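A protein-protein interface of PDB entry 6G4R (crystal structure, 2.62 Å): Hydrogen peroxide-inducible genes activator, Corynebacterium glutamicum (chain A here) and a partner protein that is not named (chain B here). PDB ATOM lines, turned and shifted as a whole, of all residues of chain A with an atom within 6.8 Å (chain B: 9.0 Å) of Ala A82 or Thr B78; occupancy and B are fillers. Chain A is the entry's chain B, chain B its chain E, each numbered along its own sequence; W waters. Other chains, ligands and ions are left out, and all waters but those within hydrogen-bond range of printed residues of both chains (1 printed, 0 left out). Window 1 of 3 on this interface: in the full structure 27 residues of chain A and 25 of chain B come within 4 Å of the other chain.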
ATOM      1  N   LEU A  10      27.318   9.548   4.979  1.00  0.00           N
ATOM      2  CA  LEU A  10      28.168   8.364   4.897  1.00  0.00           C
ATOM      3  C   LEU A  10      29.526   8.698   4.294  1.00  0.00           C
ATOM      4  O   LEU A  10      30.559   8.211   4.767  1.00  0.00           O
ATOM      5  CB  LEU A  10      27.474   7.275   4.079  1.00  0.00           C
ATOM      6  CG  LEU A  10      26.259   6.598   4.718  1.00  0.00           C
ATOM      7  CD1 LEU A  10      25.773   5.451   3.845  1.00  0.00           C
ATOM      8  CD2 LEU A  10      26.587   6.110   6.120  1.00  0.00           C
ATOM      9  N   ARG A  14      32.876   7.819   5.962  1.00  0.00           N
ATOM     10  CA  ARG A  14      33.824   6.965   5.256  1.00  0.00           C
ATOM     11  C   ARG A  14      35.196   7.621   5.165  1.00  0.00           C
ATOM     12  O   ARG A  14      36.222   6.935   5.215  1.00  0.00           O
ATOM     13  CB  ARG A  14      33.293   6.647   3.858  1.00  0.00           C
ATOM     14  CG  ARG A  14      33.983   5.487   3.163  1.00  0.00           C
ATOM     15  CD  ARG A  14      33.255   5.110   1.878  1.00  0.00           C
ATOM     16  NE  ARG A  14      31.849   4.775   2.098  1.00  0.00           N
ATOM     17  CZ  ARG A  14      30.838   5.582   1.791  1.00  0.00           C
ATOM     18  NH1 ARG A  14      31.078   6.767   1.249  1.00  0.00           N
ATOM     19  NH2 ARG A  14      29.587   5.207   2.021  1.00  0.00           N
ATOM     20  N   SER A  77      30.723   1.248  12.904  1.00  0.00           N
ATOM     21  CA  SER A  77      29.494   0.464  12.962  1.00  0.00           C
ATOM     22  C   SER A  77      28.415   1.049  12.061  1.00  0.00           C
ATOM     23  O   SER A  77      27.566   0.307  11.552  1.00  0.00           O
ATOM     24  CB  SER A  77      28.995   0.373  14.404  1.00  0.00           C
ATOM     25  OG  SER A  77      28.872   1.659  14.985  1.00  0.00           O
ATOM     26  N   THR A  78      28.426   2.367  11.855  1.00  0.00           N
ATOM     27  CA  THR A  78      27.495   2.977  10.912  1.00  0.00           C
ATOM     28  C   THR A  78      27.798   2.545   9.482  1.00  0.00           C
ATOM     29  O   THR A  78      26.878   2.257   8.706  1.00  0.00           O
ATOM     30  CB  THR A  78      27.541   4.501  11.032  1.00  0.00           C
ATOM     31  OG1 THR A  78      27.285   4.884  12.389  1.00  0.00           O
ATOM     32  CG2 THR A  78      26.497   5.141  10.129  1.00  0.00           C
ATOM     33  N   LEU A  79      29.081   2.493   9.119  1.00  0.00           N
ATOM     34  CA  LEU A  79      29.454   2.064   7.774  1.00  0.00           C
ATOM     35  C   LEU A  79      29.186   0.578   7.570  1.00  0.00           C
ATOM     36  O   LEU A  79      28.744   0.164   6.491  1.00  0.00           O
ATOM     37  CB  LEU A  79      30.928   2.380   7.517  1.00  0.00           C
ATOM     38  CG  LEU A  79      31.334   3.854   7.544  1.00  0.00           C
ATOM     39  CD1 LEU A  79      32.832   3.997   7.329  1.00  0.00           C
ATOM     40  CD2 LEU A  79      30.561   4.646   6.502  1.00  0.00           C
ATOM     41  N   ASP A  80      29.452  -0.240   8.592  1.00  0.00           N
ATOM     42  CA  ASP A  80      29.179  -1.671   8.488  1.00  0.00           C
ATOM     43  C   ASP A  80      27.690  -1.941   8.320  1.00  0.00           C
ATOM     44  O   ASP A  80      27.298  -2.872   7.605  1.00  0.00           O
ATOM     45  CB  ASP A  80      29.723  -2.401   9.716  1.00  0.00           C
ATOM     46  CG  ASP A  80      31.238  -2.376   9.787  1.00  0.00           C
ATOM     47  OD1 ASP A  80      31.885  -2.281   8.721  1.00  0.00           O
ATOM     48  OD2 ASP A  80      31.784  -2.453  10.908  1.00  0.00           O
ATOM     49  N   ALA A  81      26.843  -1.142   8.973  1.00  0.00           N
ATOM     50  CA  ALA A  81      25.401  -1.314   8.819  1.00  0.00           C
ATOM     51  C   ALA A  81      24.940  -0.919   7.423  1.00  0.00           C
ATOM     52  O   ALA A  81      24.083  -1.588   6.834  1.00  0.00           O
ATOM     53  CB  ALA A  81      24.661  -0.500   9.879  1.00  0.00           C
ATOM     54  N   ALA A  82      25.497   0.163   6.873  1.00  0.00           N
ATOM     55  CA  ALA A  82      25.123   0.581   5.526  1.00  0.00           C
ATOM     56  C   ALA A  82      25.664  -0.386   4.480  1.00  0.00           C
ATOM     57  O   ALA A  82      24.975  -0.701   3.503  1.00  0.00           O
ATOM     58  CB  ALA A  82      25.622   2.000   5.256  1.00  0.00           C
ATOM     59  N   GLU A  83      26.895  -0.869   4.671  1.00  0.00           N
ATOM     60  CA  GLU A  83      27.458  -1.848   3.748  1.00  0.00           C
ATOM     61  C   GLU A  83      26.701  -3.169   3.802  1.00  0.00           C
ATOM     62  O   GLU A  83      26.602  -3.870   2.789  1.00  0.00           O
ATOM     63  CB  GLU A  83      28.937  -2.063   4.064  1.00  0.00           C
ATOM     64  CG  GLU A  83      29.660  -3.004   3.120  1.00  0.00           C
ATOM     65  CD  GLU A  83      29.702  -2.488   1.696  1.00  0.00           C
ATOM     66  OE1 GLU A  83      28.889  -2.954   0.869  1.00  0.00           O
ATOM     67  OE2 GLU A  83      30.544  -1.613   1.405  1.00  0.00           O
ATOM     68  N   SER A  84      26.148  -3.517   4.967  1.00  0.00           N
ATOM     69  CA  SER A  84      25.318  -4.712   5.064  1.00  0.00           C
ATOM     70  C   SER A  84      23.974  -4.518   4.369  1.00  0.00           C
ATOM     71  O   SER A  84      23.396  -5.485   3.860  1.00  0.00           O
ATOM     72  CB  SER A  84      25.111  -5.088   6.529  1.00  0.00           C
ATOM     73  OG  SER A  84      24.220  -6.183   6.656  1.00  0.00           O
ATOM     74  N   PHE A  85      23.458  -3.284   4.344  1.00  0.00           N
ATOM     75  CA  PHE A  85      22.212  -3.017   3.629  1.00  0.00           C
ATOM     76  C   PHE A  85      22.397  -3.187   2.126  1.00  0.00           C
ATOM     77  O   PHE A  85      21.535  -3.760   1.450  1.00  0.00           O
ATOM     78  CB  PHE A  85      21.720  -1.604   3.950  1.00  0.00           C
ATOM     79  CG  PHE A  85      20.508  -1.184   3.160  1.00  0.00           C
ATOM     80  CD1 PHE A  85      19.236  -1.550   3.567  1.00  0.00           C
ATOM     81  CD2 PHE A  85      20.642  -0.418   2.011  1.00  0.00           C
ATOM     82  CE1 PHE A  85      18.121  -1.163   2.843  1.00  0.00           C
ATOM     83  CE2 PHE A  85      19.533  -0.032   1.281  1.00  0.00           C
ATOM     84  CZ  PHE A  85      18.271  -0.403   1.700  1.00  0.00           C
ATOM     85  N   LEU A  86      23.512  -2.688   1.587  1.00  0.00           N
ATOM     86  CA  LEU A  86      23.783  -2.856   0.163  1.00  0.00           C
ATOM     87  C   LEU A  86      24.056  -4.313  -0.187  1.00  0.00           C
ATOM     88  O   LEU A  86      23.733  -4.754  -1.296  1.00  0.00           O
ATOM     89  CB  LEU A  86      24.963  -1.977  -0.250  1.00  0.00           C
ATOM     90  CG  LEU A  86      25.251  -1.890  -1.749  1.00  0.00           C
ATOM     91  CD1 LEU A  86      24.056  -1.299  -2.471  1.00  0.00           C
ATOM     92  CD2 LEU A  86      26.501  -1.068  -2.009  1.00  0.00           C
ATOM     93  N   SER A  87      24.641  -5.072   0.743  1.00  0.00           N
ATOM     94  CA  SER A  87      24.903  -6.484   0.488  1.00  0.00           C
ATOM     95  C   SER A  87      23.607  -7.272   0.354  1.00  0.00           C
ATOM     96  O   SER A  87      23.473  -8.108  -0.547  1.00  0.00           O
ATOM     97  CB  SER A  87      25.774  -7.068   1.601  1.00  0.00           C
ATOM     98  OG  SER A  87      27.047  -6.448   1.633  1.00  0.00           O
ATOM     99  N   TYR B   6      27.355   3.024  -7.378  1.00  0.00           N
ATOM    100  CA  TYR B   6      26.283   3.576  -6.561  1.00  0.00           C
ATOM    101  C   TYR B   6      26.397   3.118  -5.112  1.00  0.00           C
ATOM    102  O   TYR B   6      26.582   1.930  -4.834  1.00  0.00           O
ATOM    103  CB  TYR B   6      24.923   3.177  -7.129  1.00  0.00           C
ATOM    104  CG  TYR B   6      23.772   3.544  -6.221  1.00  0.00           C
ATOM    105  CD1 TYR B   6      23.307   4.850  -6.152  1.00  0.00           C
ATOM    106  CD2 TYR B   6      23.155   2.585  -5.426  1.00  0.00           C
ATOM    107  CE1 TYR B   6      22.261   5.192  -5.320  1.00  0.00           C
ATOM    108  CE2 TYR B   6      22.106   2.919  -4.591  1.00  0.00           C
ATOM    109  CZ  TYR B   6      21.663   4.223  -4.543  1.00  0.00           C
ATOM    110  OH  TYR B   6      20.619   4.560  -3.713  1.00  0.00           O
ATOM    111  N   ARG B   7      26.266   4.071  -4.190  1.00  0.00           N
ATOM    112  CA  ARG B   7      26.164   3.807  -2.763  1.00  0.00           C
ATOM    113  C   ARG B   7      24.950   4.570  -2.246  1.00  0.00           C
ATOM    114  O   ARG B   7      24.779   5.755  -2.584  1.00  0.00           O
ATOM    115  CB  ARG B   7      27.428   4.241  -2.004  1.00  0.00           C
ATOM    116  CG  ARG B   7      28.741   4.009  -2.738  1.00  0.00           C
ATOM    117  CD  ARG B   7      29.037   2.531  -2.923  1.00  0.00           C
ATOM    118  NE  ARG B   7      28.902   1.784  -1.676  1.00  0.00           N
ATOM    119  CZ  ARG B   7      29.852   1.693  -0.751  1.00  0.00           C
ATOM    120  NH1 ARG B   7      31.012   2.311  -0.925  1.00  0.00           N
ATOM    121  NH2 ARG B   7      29.639   0.988   0.351  1.00  0.00           N
ATOM    122  N   PRO B   8      24.089   3.951  -1.445  1.00  0.00           N
ATOM    123  CA  PRO B   8      22.948   4.689  -0.894  1.00  0.00           C
ATOM    124  C   PRO B   8      23.397   5.678   0.171  1.00  0.00           C
ATOM    125  O   PRO B   8      24.446   5.526   0.802  1.00  0.00           O
ATOM    126  CB  PRO B   8      22.058   3.593  -0.292  1.00  0.00           C
ATOM    127  CG  PRO B   8      22.582   2.298  -0.848  1.00  0.00           C
ATOM    128  CD  PRO B   8      24.036   2.520  -1.107  1.00  0.00           C
ATOM    129  N   THR B   9      22.580   6.709   0.363  1.00  0.00           N
ATOM    130  CA  THR B   9      22.851   7.753   1.340  1.00  0.00           C
ATOM    131  C   THR B   9      21.900   7.632   2.524  1.00  0.00           C
ATOM    132  O   THR B   9      20.863   6.967   2.455  1.00  0.00           O
ATOM    133  CB  THR B   9      22.724   9.146   0.710  1.00  0.00           C
ATOM    134  OG1 THR B   9      21.342   9.441   0.468  1.00  0.00           O
ATOM    135  CG2 THR B   9      23.485   9.208  -0.606  1.00  0.00           C
ATOM    136  N   LEU B  10      22.275   8.291   3.624  1.00  0.00           N
ATOM    137  CA  LEU B  10      21.432   8.280   4.817  1.00  0.00           C
ATOM    138  C   LEU B  10      20.093   8.958   4.554  1.00  0.00           C
ATOM    139  O   LEU B  10      19.047   8.475   5.004  1.00  0.00           O
ATOM    140  CB  LEU B  10      22.156   8.958   5.980  1.00  0.00           C
ATOM    141  CG  LEU B  10      23.346   8.211   6.584  1.00  0.00           C
ATOM    142  CD1 LEU B  10      23.869   8.941   7.809  1.00  0.00           C
ATOM    143  CD2 LEU B  10      22.961   6.782   6.933  1.00  0.00           C
ATOM    144  N   ALA B  11      20.108  10.084   3.836  1.00  0.00           N
ATOM    145  CA  ALA B  11      18.866  10.789   3.531  1.00  0.00           C
ATOM    146  C   ALA B  11      17.911   9.911   2.733  1.00  0.00           C
ATOM    147  O   ALA B  11      16.691   9.965   2.933  1.00  0.00           O
ATOM    148  CB  ALA B  11      19.170  12.081   2.773  1.00  0.00           C
ATOM    149  N   LEU B  13      17.883   6.528   2.859  1.00  0.00           N
ATOM    150  CA  LEU B  13      17.406   5.529   3.809  1.00  0.00           C
ATOM    151  C   LEU B  13      16.413   6.137   4.791  1.00  0.00           C
ATOM    152  O   LEU B  13      15.404   5.508   5.129  1.00  0.00           O
ATOM    153  CB  LEU B  13      18.586   4.903   4.553  1.00  0.00           C
ATOM    154  CG  LEU B  13      19.593   4.138   3.692  1.00  0.00           C
ATOM    155  CD1 LEU B  13      20.764   3.652   4.532  1.00  0.00           C
ATOM    156  CD2 LEU B  13      18.915   2.975   2.986  1.00  0.00           C
ATOM    157  N   ARG B  14      16.689   7.357   5.262  1.00  0.00           N
ATOM    158  CA  ARG B  14      15.773   8.022   6.183  1.00  0.00           C
ATOM    159  C   ARG B  14      14.407   8.226   5.543  1.00  0.00           C
ATOM    160  O   ARG B  14      13.378   8.150   6.224  1.00  0.00           O
ATOM    161  CB  ARG B  14      16.354   9.368   6.613  1.00  0.00           C
ATOM    162  CG  ARG B  14      15.702   9.973   7.845  1.00  0.00           C
ATOM    163  CD  ARG B  14      16.450  11.215   8.312  1.00  0.00           C
ATOM    164  NE  ARG B  14      17.867  10.972   8.571  1.00  0.00           N
ATOM    165  CZ  ARG B  14      18.843  11.365   7.757  1.00  0.00           C
ATOM    166  NH1 ARG B  14      18.549  12.019   6.643  1.00  0.00           N
ATOM    167  NH2 ARG B  14      20.109  11.111   8.054  1.00  0.00           N
ATOM    168  N   VAL B  17      12.588   4.584   5.250  1.00  0.00           N
ATOM    169  CA  VAL B  17      12.065   4.077   6.517  1.00  0.00           C
ATOM    170  C   VAL B  17      10.807   4.833   6.927  1.00  0.00           C
ATOM    171  O   VAL B  17       9.815   4.227   7.352  1.00  0.00           O
ATOM    172  CB  VAL B  17      13.150   4.149   7.606  1.00  0.00           C
ATOM    173  CG1 VAL B  17      12.570   3.764   8.956  1.00  0.00           C
ATOM    174  CG2 VAL B  17      14.315   3.242   7.250  1.00  0.00           C
ATOM    175  N   LEU B  50      19.425   0.925  -6.756  1.00  0.00           N
ATOM    176  CA  LEU B  50      19.450  -0.486  -6.396  1.00  0.00           C
ATOM    177  C   LEU B  50      18.787  -1.384  -7.429  1.00  0.00           C
ATOM    178  O   LEU B  50      19.048  -2.593  -7.433  1.00  0.00           O
ATOM    179  CB  LEU B  50      18.766  -0.702  -5.040  1.00  0.00           C
ATOM    180  CG  LEU B  50      19.317   0.093  -3.856  1.00  0.00           C
ATOM    181  CD1 LEU B  50      18.473  -0.142  -2.613  1.00  0.00           C
ATOM    182  CD2 LEU B  50      20.767  -0.271  -3.601  1.00  0.00           C
ATOM    183  N   LEU B  71      14.328  -5.522   3.303  1.00  0.00           N
ATOM    184  CA  LEU B  71      15.374  -4.518   3.454  1.00  0.00           C
ATOM    185  C   LEU B  71      15.118  -3.530   4.584  1.00  0.00           C
ATOM    186  O   LEU B  71      16.075  -2.931   5.086  1.00  0.00           O
ATOM    187  CB  LEU B  71      15.556  -3.745   2.145  1.00  0.00           C
ATOM    188  CG  LEU B  71      16.169  -4.543   0.996  1.00  0.00           C
ATOM    189  CD1 LEU B  71      16.175  -3.726  -0.286  1.00  0.00           C
ATOM    190  CD2 LEU B  71      17.574  -4.981   1.366  1.00  0.00           C
ATOM    191  N   LEU B  72      13.860  -3.336   4.980  1.00  0.00           N
ATOM    192  CA  LEU B  72      13.520  -2.338   5.995  1.00  0.00           C
ATOM    193  C   LEU B  72      14.293  -2.505   7.302  1.00  0.00           C
ATOM    194  O   LEU B  72      14.779  -1.493   7.830  1.00  0.00           O
ATOM    195  CB  LEU B  72      12.000  -2.357   6.220  1.00  0.00           C
ATOM    196  CG  LEU B  72      11.337  -1.331   7.149  1.00  0.00           C
ATOM    197  CD1 LEU B  72      11.328  -1.786   8.604  1.00  0.00           C
ATOM    198  CD2 LEU B  72      11.996   0.039   7.013  1.00  0.00           C
ATOM    199  N   PRO B  73      14.436  -3.707   7.881  1.00  0.00           N
ATOM    200  CA  PRO B  73      15.225  -3.808   9.123  1.00  0.00           C
ATOM    201  C   PRO B  73      16.675  -3.386   8.951  1.00  0.00           C
ATOM    202  O   PRO B  73      17.257  -2.797   9.871  1.00  0.00           O
ATOM    203  CB  PRO B  73      15.105  -5.292   9.497  1.00  0.00           C
ATOM    204  CG  PRO B  73      13.866  -5.754   8.826  1.00  0.00           C
ATOM    205  CD  PRO B  73      13.810  -4.999   7.537  1.00  0.00           C
ATOM    206  N   PHE B  74      17.278  -3.677   7.795  1.00  0.00           N
ATOM    207  CA  PHE B  74      18.659  -3.266   7.562  1.00  0.00           C
ATOM    208  C   PHE B  74      18.781  -1.754   7.429  1.00  0.00           C
ATOM    209  O   PHE B  74      19.804  -1.179   7.820  1.00  0.00           O
ATOM    210  CB  PHE B  74      19.207  -3.954   6.311  1.00  0.00           C
ATOM    211  CG  PHE B  74      19.178  -5.453   6.383  1.00  0.00           C
ATOM    212  CD1 PHE B  74      20.124  -6.142   7.122  1.00  0.00           C
ATOM    213  CD2 PHE B  74      18.201  -6.173   5.716  1.00  0.00           C
ATOM    214  CE1 PHE B  74      20.100  -7.522   7.192  1.00  0.00           C
ATOM    215  CE2 PHE B  74      18.171  -7.554   5.783  1.00  0.00           C
ATOM    216  CZ  PHE B  74      19.122  -8.228   6.522  1.00  0.00           C
ATOM    217  N   ALA B  75      17.757  -1.094   6.883  1.00  0.00           N
ATOM    218  CA  ALA B  75      17.792   0.361   6.770  1.00  0.00           C
ATOM    219  C   ALA B  75      17.600   1.031   8.125  1.00  0.00           C
ATOM    220  O   ALA B  75      18.199   2.078   8.394  1.00  0.00           O
ATOM    221  CB  ALA B  75      16.731   0.835   5.778  1.00  0.00           C
ATOM    222  N   LYS B  76      16.773   0.442   8.993  1.00  0.00           N
ATOM    223  CA  LYS B  76      16.541   1.038  10.306  1.00  0.00           C
ATOM    224  C   LYS B  76      17.760   0.889  11.207  1.00  0.00           C
ATOM    225  O   LYS B  76      18.087   1.804  11.972  1.00  0.00           O
ATOM    226  CB  LYS B  76      15.311   0.413  10.963  1.00  0.00           C
ATOM    227  CG  LYS B  76      14.006   0.703  10.246  1.00  0.00           C
ATOM    228  CD  LYS B  76      12.811   0.365  11.121  1.00  0.00           C
ATOM    229  CE  LYS B  76      12.816   1.186  12.401  1.00  0.00           C
ATOM    230  NZ  LYS B  76      11.609   0.923  13.235  1.00  0.00           N
ATOM    231  N   SER B  77      18.444  -0.255  11.133  1.00  0.00           N
ATOM    232  CA  SER B  77      19.662  -0.431  11.915  1.00  0.00           C
ATOM    233  C   SER B  77      20.764   0.509  11.448  1.00  0.00           C
ATOM    234  O   SER B  77      21.623   0.901  12.245  1.00  0.00           O
ATOM    235  CB  SER B  77      20.130  -1.883  11.843  1.00  0.00           C
ATOM    236  OG  SER B  77      20.257  -2.310  10.499  1.00  0.00           O
ATOM    237  N   THR B  78      20.759   0.875  10.163  1.00  0.00           N
ATOM    238  CA  THR B  78      21.706   1.873   9.675  1.00  0.00           C
ATOM    239  C   THR B  78      21.421   3.243  10.278  1.00  0.00           C
ATOM    240  O   THR B  78      22.348   3.963  10.664  1.00  0.00           O
ATOM    241  CB  THR B  78      21.659   1.939   8.148  1.00  0.00           C
ATOM    242  OG1 THR B  78      21.897   0.636   7.602  1.00  0.00           O
ATOM    243  CG2 THR B  78      22.715   2.901   7.623  1.00  0.00           C
ATOM    244  N   LEU B  79      20.140   3.617  10.371  1.00  0.00           N
ATOM    245  CA  LEU B  79      19.783   4.907  10.952  1.00  0.00           C
ATOM    246  C   LEU B  79      20.050   4.935  12.451  1.00  0.00           C
ATOM    247  O   LEU B  79      20.502   5.955  12.986  1.00  0.00           O
ATOM    248  CB  LEU B  79      18.315   5.223  10.668  1.00  0.00           C
ATOM    249  CG  LEU B  79      17.916   5.379   9.202  1.00  0.00           C
ATOM    250  CD1 LEU B  79      16.423   5.642   9.088  1.00  0.00           C
ATOM    251  CD2 LEU B  79      18.713   6.494   8.546  1.00  0.00           C
ATOM    252  N   ASP B  80      19.768   3.833  13.147  1.00  0.00           N
ATOM    253  CA  ASP B  80      20.050   3.775  14.578  1.00  0.00           C
ATOM    254  C   ASP B  80      21.544   3.903  14.844  1.00  0.00           C
ATOM    255  O   ASP B  80      21.955   4.501  15.846  1.00  0.00           O
ATOM    256  CB  ASP B  80      19.503   2.477  15.172  1.00  0.00           C
ATOM    257  CG  ASP B  80      17.989   2.419  15.150  1.00  0.00           C
ATOM    258  OD1 ASP B  80      17.353   3.494  15.178  1.00  0.00           O
ATOM    259  OD2 ASP B  80      17.435   1.300  15.109  1.00  0.00           O
ATOM    260  N   ALA B  81      22.373   3.346  13.960  1.00  0.00           N
ATOM    261  CA  ALA B  81      23.816   3.488  14.109  1.00  0.00           C
ATOM    262  C   ALA B  81      24.262   4.923  13.850  1.00  0.00           C
ATOM    263  O   ALA B  81      25.140   5.441  14.549  1.00  0.00           O
ATOM    264  CB  ALA B  81      24.539   2.517  13.175  1.00  0.00           C
ATOM    265  N   ALA B  82      23.671   5.583  12.850  1.00  0.00           N
ATOM    266  CA  ALA B  82      24.031   6.971  12.579  1.00  0.00           C
ATOM    267  C   ALA B  82      23.519   7.892  13.679  1.00  0.00           C
ATOM    268  O   ALA B  82      24.217   8.829  14.084  1.00  0.00           O
ATOM    269  CB  ALA B  82      23.491   7.402  11.216  1.00  0.00           C
ATOM    270  N   GLU B  83      22.304   7.642  14.173  1.00  0.00           N
ATOM    271  CA  GLU B  83      21.792   8.419  15.296  1.00  0.00           C
ATOM    272  C   GLU B  83      22.599   8.166  16.561  1.00  0.00           C
ATOM    273  O   GLU B  83      22.699   9.051  17.417  1.00  0.00           O
ATOM    274  CB  GLU B  83      20.308   8.105  15.520  1.00  0.00           C
ATOM    275  CG  GLU B  83      19.649   8.879  16.659  1.00  0.00           C
ATOM    276  CD  GLU B  83      19.365  10.330  16.310  1.00  0.00           C
ATOM    277  OE1 GLU B  83      19.601  10.729  15.150  1.00  0.00           O
ATOM    278  OE2 GLU B  83      18.899  11.071  17.199  1.00  0.00           O
ATOM    279  N   SER B  84      23.178   6.971  16.694  1.00  0.00           N
ATOM    280  CA  SER B  84      24.044   6.697  17.835  1.00  0.00           C
ATOM    281  C   SER B  84      25.357   7.456  17.731  1.00  0.00           C
ATOM    282  O   SER B  84      25.951   7.803  18.755  1.00  0.00           O
ATOM    283  CB  SER B  84      24.337   5.199  17.965  1.00  0.00           C
ATOM    284  OG  SER B  84      25.020   4.711  16.819  1.00  0.00           O
ATOM    285  N   PHE B  85      25.832   7.701  16.508  1.00  0.00           N
ATOM    286  CA  PHE B  85      27.051   8.484  16.322  1.00  0.00           C
ATOM    287  C   PHE B  85      26.837   9.948  16.699  1.00  0.00           C
ATOM    288  O   PHE B  85      27.693  10.555  17.355  1.00  0.00           O
ATOM    289  CB  PHE B  85      27.537   8.361  14.875  1.00  0.00           C
ATOM    290  CG  PHE B  85      28.726   9.237  14.552  1.00  0.00           C
ATOM    291  CD1 PHE B  85      30.011   8.831  14.872  1.00  0.00           C
ATOM    292  CD2 PHE B  85      28.561  10.455  13.904  1.00  0.00           C
ATOM    293  CE1 PHE B  85      31.109   9.629  14.575  1.00  0.00           C
ATOM    294  CE2 PHE B  85      29.657  11.258  13.602  1.00  0.00           C
ATOM    295  CZ  PHE B  85      30.932  10.842  13.939  1.00  0.00           C
HETATM  296  O   HOH W   1      25.108   9.472   3.103  1.00  0.00           O
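O of Ala A81 sits at hydrogen-bond distance from OG1 of Thr B78, at 3.2 Å.
OE2 of Glu A83 lies within salt-bridge range of NH2 of Arg B7 (2.9 Å).
The backbone carbonyl oxygen of Ala B81 lies within hydrogen-bond range of the side-chain hydroxyl of Thr A78 (3.1 Å).
The side-chain hydroxyl (OG) of Ser B77 sits at hydrogen-bond distance from the backbone carbonyl oxygen (O) of Phe B74, at 2.9 Å.
The backbone carbonyl oxygen (O) of Glu A83 lies within hydrogen-bond range of the side-chain hydroxyl (OG) of Ser A87, 2.9 Å away.
OG1 of Thr B78 is in hydrogen-bond range of O of Phe B74 (2.8 Å).
Among the printed residues, pairs that only touch across the chains: Leu A10 with Pro B8 (3.3 Å), Leu A10 with Leu B10 (3.8 Å), Arg A14 with Arg B7 (3.99 Å), Thr A78 with Ala B82 (3.7 Å), Ala A82 with Thr B78 (3.7 Å), Phe A85 with Leu B13 (3.5 Å), Phe A85 with Leu B71 (3.5 Å), Phe A85 with Phe B74 (3.6 Å), Phe A85 with Ala B75 (3.7 Å), Leu A86 with Arg B7 (3.7 Å) and Leu A86 with Leu B50 (3.6 Å).
Printed residues of chain B within 4 Å of Leu A10: Pro B8 (3.3 Å) and Leu B10 (3.8 Å).
Of chain B, only Thr B78 (3.2 Å) comes within 4 Å of Ala A81.
Ala A82 touches just one residue of chain B: Thr B78 (3.7 Å).
Ser A84 touches none of the printed residues of chain B.
Of the printed residues of chain A, Leu B10 touches Leu A10 (3.8 Å).
Printed residues of chain A within 4 Å of Leu B50: Leu A86 (3.6 Å).
Lys B76 touches none of the printed residues of chain A.
Thr B78 touches two residues of chain A.
Printed residues of chain A within 4 Å of Ala B81: Thr A78.
The nearest residue of chain A that does not touch Thr B78 is Phe A85 (4.3 Å).
The nearest printed residue of chain B that does not touch Arg A14 is Pro B8 (5.3 Å).
Printed residues of chain B that touch a printed residue of chain A: Arg B7, Pro B8, Leu B10, Leu B13, Leu B50, Leu B71, Phe B74, Ala B75, Thr B78, Ala B81 and Ala B82.
Hydrophobic or aromatic side chains of chain B within 4 Å of the printed part of chain A: Leu B10, Leu B13, Leu B50, Leu B71, Phe B74, Ala B75, Ala B81 and Ala B82.
Among the printed residues, Asp or Glu carboxylates within 4 Å of a Lys or Arg side-chain nitrogen of the other chain: Glu A83 with Arg B7.
Water W1 bridges the backbone NH (N) of Leu A10 (2.9 Å) and the backbone NH (N) of Leu B10 (3.1 Å).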
